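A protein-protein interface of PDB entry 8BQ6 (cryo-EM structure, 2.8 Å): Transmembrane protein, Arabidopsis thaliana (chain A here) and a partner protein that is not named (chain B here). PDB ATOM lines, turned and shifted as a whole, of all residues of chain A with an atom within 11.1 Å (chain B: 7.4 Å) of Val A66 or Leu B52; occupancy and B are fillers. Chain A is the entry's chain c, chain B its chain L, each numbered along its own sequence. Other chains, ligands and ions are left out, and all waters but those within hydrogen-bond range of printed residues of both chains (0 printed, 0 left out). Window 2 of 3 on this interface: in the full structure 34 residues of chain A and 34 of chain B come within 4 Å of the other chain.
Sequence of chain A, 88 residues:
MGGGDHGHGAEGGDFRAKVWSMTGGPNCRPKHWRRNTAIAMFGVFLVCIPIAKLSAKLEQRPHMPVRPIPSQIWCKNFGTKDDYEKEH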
ATOM      1  N   ARG A  61     -25.002 -23.068  -0.345  1.00  0.00           N
ATOM      2  CA  ARG A  61     -23.781 -22.271  -0.642  1.00  0.00           C
ATOM      3  C   ARG A  61     -22.993 -22.988  -1.743  1.00  0.00           C
ATOM      4  O   ARG A  61     -22.159 -23.844  -1.406  1.00  0.00           O
ATOM      5  CB  ARG A  61     -22.930 -22.077   0.617  1.00  0.00           C
ATOM      6  CG  ARG A  61     -23.723 -21.965   1.910  1.00  0.00           C
ATOM      7  CD  ARG A  61     -24.199 -20.554   2.187  1.00  0.00           C
ATOM      8  NE  ARG A  61     -23.148 -19.546   2.153  1.00  0.00           N
ATOM      9  CZ  ARG A  61     -22.726 -18.866   3.215  1.00  0.00           C
ATOM     10  NH1 ARG A  61     -23.263 -19.091   4.402  1.00  0.00           N
ATOM     11  NH2 ARG A  61     -21.770 -17.965   3.089  1.00  0.00           N
ATOM     12  N   PRO A  62     -23.204 -22.668  -3.039  1.00  0.00           N
ATOM     13  CA  PRO A  62     -22.550 -23.390  -4.138  1.00  0.00           C
ATOM     14  C   PRO A  62     -21.057 -23.148  -4.215  1.00  0.00           C
ATOM     15  O   PRO A  62     -20.383 -23.800  -5.020  1.00  0.00           O
ATOM     16  CB  PRO A  62     -23.266 -22.853  -5.389  1.00  0.00           C
ATOM     17  CG  PRO A  62     -24.449 -22.066  -4.871  1.00  0.00           C
ATOM     18  CD  PRO A  62     -24.034 -21.563  -3.536  1.00  0.00           C
ATOM     19  N   HIS A  63     -20.555 -22.225  -3.402  1.00  0.00           N
ATOM     20  CA  HIS A  63     -19.135 -21.834  -3.495  1.00  0.00           C
ATOM     21  C   HIS A  63     -18.427 -21.983  -2.156  1.00  0.00           C
ATOM     22  O   HIS A  63     -18.960 -21.486  -1.142  1.00  0.00           O
ATOM     23  CB  HIS A  63     -19.059 -20.383  -3.961  1.00  0.00           C
ATOM     24  CG  HIS A  63     -19.139 -20.230  -5.437  1.00  0.00           C
ATOM     25  ND1 HIS A  63     -18.610 -21.166  -6.298  1.00  0.00           N
ATOM     26  CD2 HIS A  63     -19.683 -19.263  -6.204  1.00  0.00           C
ATOM     27  CE1 HIS A  63     -18.817 -20.780  -7.537  1.00  0.00           C
ATOM     28  NE2 HIS A  63     -19.475 -19.616  -7.506  1.00  0.00           N
ATOM     29  N   MET A  64     -17.281 -22.656  -2.152  1.00  0.00           N
ATOM     30  CA  MET A  64     -16.456 -22.735  -0.957  1.00  0.00           C
ATOM     31  C   MET A  64     -15.900 -21.353  -0.628  1.00  0.00           C
ATOM     32  O   MET A  64     -15.408 -20.659  -1.527  1.00  0.00           O
ATOM     33  CB  MET A  64     -15.315 -23.727  -1.168  1.00  0.00           C
ATOM     34  CG  MET A  64     -15.787 -25.121  -1.529  1.00  0.00           C
ATOM     35  SD  MET A  64     -16.220 -26.077  -0.066  1.00  0.00           S
ATOM     36  CE  MET A  64     -16.645 -27.650  -0.806  1.00  0.00           C
ATOM     37  N   PRO A  65     -16.010 -20.872   0.644  1.00  0.00           N
ATOM     38  CA  PRO A  65     -15.445 -19.581   1.003  1.00  0.00           C
ATOM     39  C   PRO A  65     -13.920 -19.557   0.904  1.00  0.00           C
ATOM     40  O   PRO A  65     -13.280 -20.595   0.997  1.00  0.00           O
ATOM     41  CB  PRO A  65     -15.862 -19.355   2.458  1.00  0.00           C
ATOM     42  CG  PRO A  65     -16.017 -20.733   2.992  1.00  0.00           C
ATOM     43  CD  PRO A  65     -16.692 -21.439   1.845  1.00  0.00           C
ATOM     44  N   VAL A  66     -13.373 -18.360   0.747  1.00  0.00           N
ATOM     45  CA  VAL A  66     -11.926 -18.203   0.646  1.00  0.00           C
ATOM     46  C   VAL A  66     -11.246 -18.578   1.960  1.00  0.00           C
ATOM     47  O   VAL A  66     -10.090 -19.018   1.971  1.00  0.00           O
ATOM     48  CB  VAL A  66     -11.571 -16.771   0.202  1.00  0.00           C
ATOM     49  CG1 VAL A  66     -12.489 -16.322  -0.922  1.00  0.00           C
ATOM     50  CG2 VAL A  66     -11.632 -15.800   1.371  1.00  0.00           C
ATOM     51  N   ARG A  67     -11.936 -18.403   3.079  1.00  0.00           N
ATOM     52  CA  ARG A  67     -11.458 -18.766   4.403  1.00  0.00           C
ATOM     53  C   ARG A  67     -12.596 -19.412   5.177  1.00  0.00           C
ATOM     54  O   ARG A  67     -13.769 -19.219   4.840  1.00  0.00           O
ATOM     55  CB  ARG A  67     -10.924 -17.544   5.166  1.00  0.00           C
ATOM     56  CG  ARG A  67     -11.863 -16.351   5.224  1.00  0.00           C
ATOM     57  CD  ARG A  67     -11.212 -15.210   5.989  1.00  0.00           C
ATOM     58  NE  ARG A  67     -10.232 -14.492   5.182  1.00  0.00           N
ATOM     59  CZ  ARG A  67     -10.543 -13.568   4.283  1.00  0.00           C
ATOM     60  NH1 ARG A  67     -11.801 -13.229   4.050  1.00  0.00           N
ATOM     61  NH2 ARG A  67      -9.569 -12.966   3.607  1.00  0.00           N
ATOM     62  N   PRO A  68     -12.287 -20.205   6.205  1.00  0.00           N
ATOM     63  CA  PRO A  68     -13.358 -20.842   6.981  1.00  0.00           C
ATOM     64  C   PRO A  68     -14.293 -19.812   7.597  1.00  0.00           C
ATOM     65  O   PRO A  68     -13.865 -18.756   8.069  1.00  0.00           O
ATOM     66  CB  PRO A  68     -12.599 -21.627   8.053  1.00  0.00           C
ATOM     67  CG  PRO A  68     -11.290 -21.924   7.418  1.00  0.00           C
ATOM     68  CD  PRO A  68     -10.959 -20.680   6.636  1.00  0.00           C
ATOM     69  N   ILE A  69     -15.582 -20.139   7.599  1.00  0.00           N
ATOM     70  CA  ILE A  69     -16.623 -19.196   7.998  1.00  0.00           C
ATOM     71  C   ILE A  69     -17.527 -19.878   9.017  1.00  0.00           C
ATOM     72  O   ILE A  69     -17.652 -21.113   9.028  1.00  0.00           O
ATOM     73  CB  ILE A  69     -17.436 -18.706   6.780  1.00  0.00           C
ATOM     74  CG1 ILE A  69     -17.970 -19.901   5.991  1.00  0.00           C
ATOM     75  CG2 ILE A  69     -16.589 -17.804   5.897  1.00  0.00           C
ATOM     76  CD1 ILE A  69     -19.012 -19.545   4.957  1.00  0.00           C
ATOM     77  N   PRO A  70     -18.193 -19.096   9.876  1.00  0.00           N
ATOM     78  CA  PRO A  70     -18.995 -19.708  10.951  1.00  0.00           C
ATOM     79  C   PRO A  70     -20.123 -20.596  10.462  1.00  0.00           C
ATOM     80  O   PRO A  70     -20.630 -21.415  11.239  1.00  0.00           O
ATOM     81  CB  PRO A  70     -19.545 -18.494  11.710  1.00  0.00           C
ATOM     82  CG  PRO A  70     -18.607 -17.393  11.400  1.00  0.00           C
ATOM     83  CD  PRO A  70     -18.154 -17.629   9.993  1.00  0.00           C
ATOM     84  N   SER A  71     -20.561 -20.446   9.212  1.00  0.00           N
ATOM     85  CA  SER A  71     -21.671 -21.264   8.743  1.00  0.00           C
ATOM     86  C   SER A  71     -21.215 -22.631   8.261  1.00  0.00           C
ATOM     87  O   SER A  71     -22.053 -23.447   7.873  1.00  0.00           O
ATOM     88  CB  SER A  71     -22.433 -20.548   7.633  1.00  0.00           C
ATOM     89  OG  SER A  71     -21.549 -19.945   6.713  1.00  0.00           O
ATOM     90  N   GLN A  72     -19.911 -22.900   8.267  1.00  0.00           N
ATOM     91  CA  GLN A  72     -19.441 -24.251   7.992  1.00  0.00           C
ATOM     92  C   GLN A  72     -19.540 -25.142   9.218  1.00  0.00           C
ATOM     93  O   GLN A  72     -19.277 -26.344   9.126  1.00  0.00           O
ATOM     94  CB  GLN A  72     -18.006 -24.207   7.480  1.00  0.00           C
ATOM     95  CG  GLN A  72     -17.920 -23.864   6.012  1.00  0.00           C
ATOM     96  CD  GLN A  72     -16.521 -23.511   5.584  1.00  0.00           C
ATOM     97  OE1 GLN A  72     -15.723 -23.021   6.380  1.00  0.00           O
ATOM     98  NE2 GLN A  72     -16.212 -23.751   4.318  1.00  0.00           N
ATOM     99  N   PHE A  78     -22.353 -27.043   1.230  1.00  0.00           N
ATOM    100  CA  PHE A  78     -21.282 -26.265   0.558  1.00  0.00           C
ATOM    101  C   PHE A  78     -20.771 -27.039  -0.654  1.00  0.00           C
ATOM    102  O   PHE A  78     -20.436 -28.229  -0.512  1.00  0.00           O
ATOM    103  CB  PHE A  78     -20.166 -25.945   1.552  1.00  0.00           C
ATOM    104  CG  PHE A  78     -20.441 -24.796   2.488  1.00  0.00           C
ATOM    105  CD1 PHE A  78     -21.233 -24.966   3.612  1.00  0.00           C
ATOM    106  CD2 PHE A  78     -19.891 -23.548   2.250  1.00  0.00           C
ATOM    107  CE1 PHE A  78     -21.481 -23.907   4.470  1.00  0.00           C
ATOM    108  CE2 PHE A  78     -20.139 -22.491   3.111  1.00  0.00           C
ATOM    109  CZ  PHE A  78     -20.935 -22.672   4.218  1.00  0.00           C
ATOM    110  N   LEU B  44     -23.458  -8.398  10.187  1.00  0.00           N
ATOM    111  CA  LEU B  44     -22.015  -8.212  10.078  1.00  0.00           C
ATOM    112  C   LEU B  44     -21.316  -9.529   9.780  1.00  0.00           C
ATOM    113  O   LEU B  44     -20.354  -9.573   9.005  1.00  0.00           O
ATOM    114  CB  LEU B  44     -21.474  -7.611  11.372  1.00  0.00           C
ATOM    115  CG  LEU B  44     -21.804  -6.145  11.631  1.00  0.00           C
ATOM    116  CD1 LEU B  44     -21.241  -5.723  12.973  1.00  0.00           C
ATOM    117  CD2 LEU B  44     -21.272  -5.265  10.518  1.00  0.00           C
ATOM    118  N   ALA B  46     -22.769 -11.971   8.210  1.00  0.00           N
ATOM    119  CA  ALA B  46     -23.159 -12.324   6.849  1.00  0.00           C
ATOM    120  C   ALA B  46     -22.360 -11.533   5.818  1.00  0.00           C
ATOM    121  O   ALA B  46     -22.091 -12.032   4.720  1.00  0.00           O
ATOM    122  CB  ALA B  46     -24.659 -12.104   6.661  1.00  0.00           C
ATOM    123  N   PHE B  47     -21.991 -10.293   6.145  1.00  0.00           N
ATOM    124  CA  PHE B  47     -21.135  -9.514   5.256  1.00  0.00           C
ATOM    125  C   PHE B  47     -19.748 -10.130   5.148  1.00  0.00           C
ATOM    126  O   PHE B  47     -19.170 -10.202   4.056  1.00  0.00           O
ATOM    127  CB  PHE B  47     -21.051  -8.073   5.757  1.00  0.00           C
ATOM    128  CG  PHE B  47     -20.149  -7.196   4.941  1.00  0.00           C
ATOM    129  CD1 PHE B  47     -20.623  -6.580   3.800  1.00  0.00           C
ATOM    130  CD2 PHE B  47     -18.842  -6.956   5.335  1.00  0.00           C
ATOM    131  CE1 PHE B  47     -19.807  -5.765   3.044  1.00  0.00           C
ATOM    132  CE2 PHE B  47     -18.018  -6.137   4.585  1.00  0.00           C
ATOM    133  CZ  PHE B  47     -18.504  -5.539   3.438  1.00  0.00           C
ATOM    134  N   TYR B  48     -19.198 -10.569   6.276  1.00  0.00           N
ATOM    135  CA  TYR B  48     -17.923 -11.275   6.272  1.00  0.00           C
ATOM    136  C   TYR B  48     -18.011 -12.563   5.465  1.00  0.00           C
ATOM    137  O   TYR B  48     -17.105 -12.885   4.689  1.00  0.00           O
ATOM    138  CB  TYR B  48     -17.522 -11.550   7.719  1.00  0.00           C
ATOM    139  CG  TYR B  48     -16.263 -12.344   7.929  1.00  0.00           C
ATOM    140  CD1 TYR B  48     -15.034 -11.713   8.054  1.00  0.00           C
ATOM    141  CD2 TYR B  48     -16.309 -13.725   8.051  1.00  0.00           C
ATOM    142  CE1 TYR B  48     -13.885 -12.438   8.268  1.00  0.00           C
ATOM    143  CE2 TYR B  48     -15.167 -14.457   8.265  1.00  0.00           C
ATOM    144  CZ  TYR B  48     -13.959 -13.809   8.375  1.00  0.00           C
ATOM    145  OH  TYR B  48     -12.821 -14.544   8.591  1.00  0.00           O
ATOM    146  N   GLU B  49     -19.066 -13.367   5.616  1.00  0.00           N
ATOM    147  CA  GLU B  49     -19.035 -14.688   4.912  1.00  0.00           C
ATOM    148  C   GLU B  49     -19.394 -14.578   3.428  1.00  0.00           C
ATOM    149  O   GLU B  49     -18.889 -15.409   2.654  1.00  0.00           O
ATOM    150  CB  GLU B  49     -19.966 -15.721   5.536  1.00  0.00           C
ATOM    151  CG  GLU B  49     -19.853 -15.861   7.032  1.00  0.00           C
ATOM    152  CD  GLU B  49     -21.104 -16.492   7.611  1.00  0.00           C
ATOM    153  OE1 GLU B  49     -22.190 -15.919   7.418  1.00  0.00           O
ATOM    154  OE2 GLU B  49     -20.990 -17.559   8.232  1.00  0.00           O
ATOM    155  N   VAL B  50     -20.237 -13.623   3.041  1.00  0.00           N
ATOM    156  CA  VAL B  50     -20.713 -13.573   1.625  1.00  0.00           C
ATOM    157  C   VAL B  50     -19.828 -12.623   0.819  1.00  0.00           C
ATOM    158  O   VAL B  50     -19.449 -12.991  -0.302  1.00  0.00           O
ATOM    159  CB  VAL B  50     -22.205 -13.172   1.535  1.00  0.00           C
ATOM    160  CG1 VAL B  50     -22.656 -12.963   0.104  1.00  0.00           C
ATOM    161  CG2 VAL B  50     -23.116 -14.165   2.237  1.00  0.00           C
ATOM    162  N   ALA B  51     -19.534 -11.439   1.352  1.00  0.00           N
ATOM    163  CA  ALA B  51     -18.771 -10.474   0.570  1.00  0.00           C
ATOM    164  C   ALA B  51     -17.271 -10.695   0.723  1.00  0.00           C
ATOM    165  O   ALA B  51     -16.537 -10.771  -0.268  1.00  0.00           O
ATOM    166  CB  ALA B  51     -19.148  -9.050   0.983  1.00  0.00           C
ATOM    167  N   LEU B  52     -16.797 -10.786   1.967  1.00  0.00           N
ATOM    168  CA  LEU B  52     -15.370 -10.976   2.199  1.00  0.00           C
ATOM    169  C   LEU B  52     -14.942 -12.402   1.885  1.00  0.00           C
ATOM    170  O   LEU B  52     -13.845 -12.626   1.361  1.00  0.00           O
ATOM    171  CB  LEU B  52     -15.026 -10.613   3.642  1.00  0.00           C
ATOM    172  CG  LEU B  52     -15.448  -9.205   4.055  1.00  0.00           C
ATOM    173  CD1 LEU B  52     -15.021  -8.910   5.480  1.00  0.00           C
ATOM    174  CD2 LEU B  52     -14.863  -8.187   3.095  1.00  0.00           C
ATOM    175  N   GLY B  53     -15.799 -13.379   2.192  1.00  0.00           N
ATOM    176  CA  GLY B  53     -15.467 -14.795   1.949  1.00  0.00           C
ATOM    177  C   GLY B  53     -15.878 -15.265   0.568  1.00  0.00           C
ATOM    178  O   GLY B  53     -15.610 -16.429   0.265  1.00  0.00           O
ATOM    179  N   ALA B  54     -16.515 -14.408  -0.231  1.00  0.00           N
ATOM    180  CA  ALA B  54     -17.017 -14.778  -1.581  1.00  0.00           C
ATOM    181  C   ALA B  54     -17.785 -16.108  -1.543  1.00  0.00           C
ATOM    182  O   ALA B  54     -17.384 -17.033  -2.277  1.00  0.00           O
ATOM    183  CB  ALA B  54     -15.884 -14.798  -2.580  1.00  0.00           C
ATOM    184  N   SER B  55     -18.853 -16.191  -0.745  1.00  0.00           N
ATOM    185  CA  SER B  55     -19.718 -17.402  -0.699  1.00  0.00           C
ATOM    186  C   SER B  55     -21.182 -16.958  -0.601  1.00  0.00           C
ATOM    187  O   SER B  55     -21.620 -16.635   0.510  1.00  0.00           O
ATOM    188  CB  SER B  55     -19.355 -18.303   0.449  1.00  0.00           C
ATOM    189  OG  SER B  55     -20.196 -19.445   0.481  1.00  0.00           O
ATOM    190  N   SER B  80     -23.371 -10.104  -2.727  1.00  0.00           N
ATOM    191  CA  SER B  80     -22.580  -8.971  -2.263  1.00  0.00           C
ATOM    192  C   SER B  80     -23.425  -7.709  -2.141  1.00  0.00           C
ATOM    193  O   SER B  80     -23.271  -6.937  -1.188  1.00  0.00           O
ATOM    194  CB  SER B  80     -21.402  -8.749  -3.207  1.00  0.00           C
ATOM    195  OG  SER B  80     -20.391  -9.702  -2.948  1.00  0.00           O
ATOM    196  N   VAL B  83     -25.753  -8.066   1.145  1.00  0.00           N
ATOM    197  CA  VAL B  83     -25.145  -7.900   2.460  1.00  0.00           C
ATOM    198  C   VAL B  83     -24.655  -6.476   2.666  1.00  0.00           C
ATOM    199  O   VAL B  83     -24.427  -6.053   3.805  1.00  0.00           O
ATOM    200  CB  VAL B  83     -24.009  -8.920   2.657  1.00  0.00           C
ATOM    201  CG1 VAL B  83     -24.579 -10.316   2.777  1.00  0.00           C
ATOM    202  CG2 VAL B  83     -23.023  -8.839   1.506  1.00  0.00           C
ATOM    203  N   MET B 484     -12.565  -1.506  -1.827  1.00  0.00           N
ATOM    204  CA  MET B 484     -13.543  -2.584  -1.791  1.00  0.00           C
ATOM    205  C   MET B 484     -14.648  -2.367  -2.818  1.00  0.00           C
ATOM    206  O   MET B 484     -14.928  -3.252  -3.632  1.00  0.00           O
ATOM    207  CB  MET B 484     -14.141  -2.702  -0.393  1.00  0.00           C
ATOM    208  CG  MET B 484     -14.454  -4.115   0.021  1.00  0.00           C
ATOM    209  SD  MET B 484     -15.469  -4.157   1.502  1.00  0.00           S
ATOM    210  CE  MET B 484     -16.669  -2.889   1.101  1.00  0.00           C
ATOM    211  N   PHE B 492     -15.225  -7.411  -5.777  1.00  0.00           N
ATOM    212  CA  PHE B 492     -16.013  -7.468  -4.551  1.00  0.00           C
ATOM    213  C   PHE B 492     -17.467  -7.811  -4.838  1.00  0.00           C
ATOM    214  O   PHE B 492     -18.102  -8.558  -4.085  1.00  0.00           O
ATOM    215  CB  PHE B 492     -15.893  -6.129  -3.831  1.00  0.00           C
ATOM    216  CG  PHE B 492     -16.854  -5.944  -2.699  1.00  0.00           C
ATOM    217  CD1 PHE B 492     -16.671  -6.602  -1.501  1.00  0.00           C
ATOM    218  CD2 PHE B 492     -17.924  -5.077  -2.828  1.00  0.00           C
ATOM    219  CE1 PHE B 492     -17.547  -6.411  -0.459  1.00  0.00           C
ATOM    220  CE2 PHE B 492     -18.804  -4.887  -1.788  1.00  0.00           C
ATOM    221  CZ  PHE B 492     -18.615  -5.553  -0.603  1.00  0.00           C
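O of Tyr B48 sits at hydrogen-bond distance from N of Gly B53, 2.9 Å away.
O of Val B50 is in hydrogen-bond range of N of Ser B55 (3.3 Å).
N of Ser B55 lies within hydrogen-bond range of O of Glu B49 (3.5 Å).
OE1 of Gln A72 sits at hydrogen-bond distance from N of Ile A69 (3.1 Å).
The backbone carbonyl oxygen (O) of Phe B47 lies within hydrogen-bond range of the backbone NH (N) of Leu B52, 3.2 Å away.
NH1 of Arg A61 lies within hydrogen-bond range of OG of Ser A71 (3.0 Å).
The backbone carbonyl oxygen (O) of Gly B53 sits at hydrogen-bond distance from the backbone NH (N) of Val A66 (3.0 Å).
The backbone carbonyl oxygen of His A63 is in hydrogen-bond range of the side-chain hydroxyl of Ser B55 (2.9 Å).
O of Ser B55 is in hydrogen-bond range of NH2 of Arg A61 (2.9 Å).
The side-chain carboxylate of Glu B49 is in hydrogen-bond range of the side-chain hydroxyl of Ser A71 (2.9 Å).
NH1 of Arg A67 lies within hydrogen-bond range of O of Leu B52 (3.4 Å).
Among the printed residues, pairs that only touch across the chains: Arg A61 with Glu B49, Pro A65 with Gly B53, Val A66 with Leu B52, Arg A67 with Tyr B48, Ile A69 with Glu B49 and Pro A70 with Glu B49.
Of the 15 printed residues of chain B, 5 touch a printed residue of chain A.
Hydrophobic or aromatic side chains of chain B that line the printed part of chain A: Tyr B48.
Printed residues of chain A that touch a printed residue of chain B: Arg A61, His A63, Pro A65, Val A66, Arg A67, Ile A69, Pro A70 and Ser A71.
Hydrophobic or aromatic side chains of chain A within 4 Å of the printed part of chain B: Pro A65, Val A66, Ile A69 and Pro A70.
Of chain B, only Leu B52 and Gly B53 come within 4 Å of Val A66.
Of chain A, only Val A66 and Arg A67 come within 4 Å of Leu B52.
No residue of chain A comes within 4 Å of Phe B47.
Tyr B48 touches just one residue of chain A: Arg A67.
Of chain A, only Pro A65 and Val A66 come within 4 Å of Gly B53.
Ala B54 touches none of the printed residues of chain A.
Of the printed residues of chain A, Glu B49 touches Arg A61, Ile A69, Pro A70 and Ser A71.
Printed residues of chain B within 4 Å of Ser A71: Glu B49 (2.9 Å).
Of the printed residues of chain B, Pro A70 touches Glu B49 (3.3 Å).
Met A64 touches none of the printed residues of chain B.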
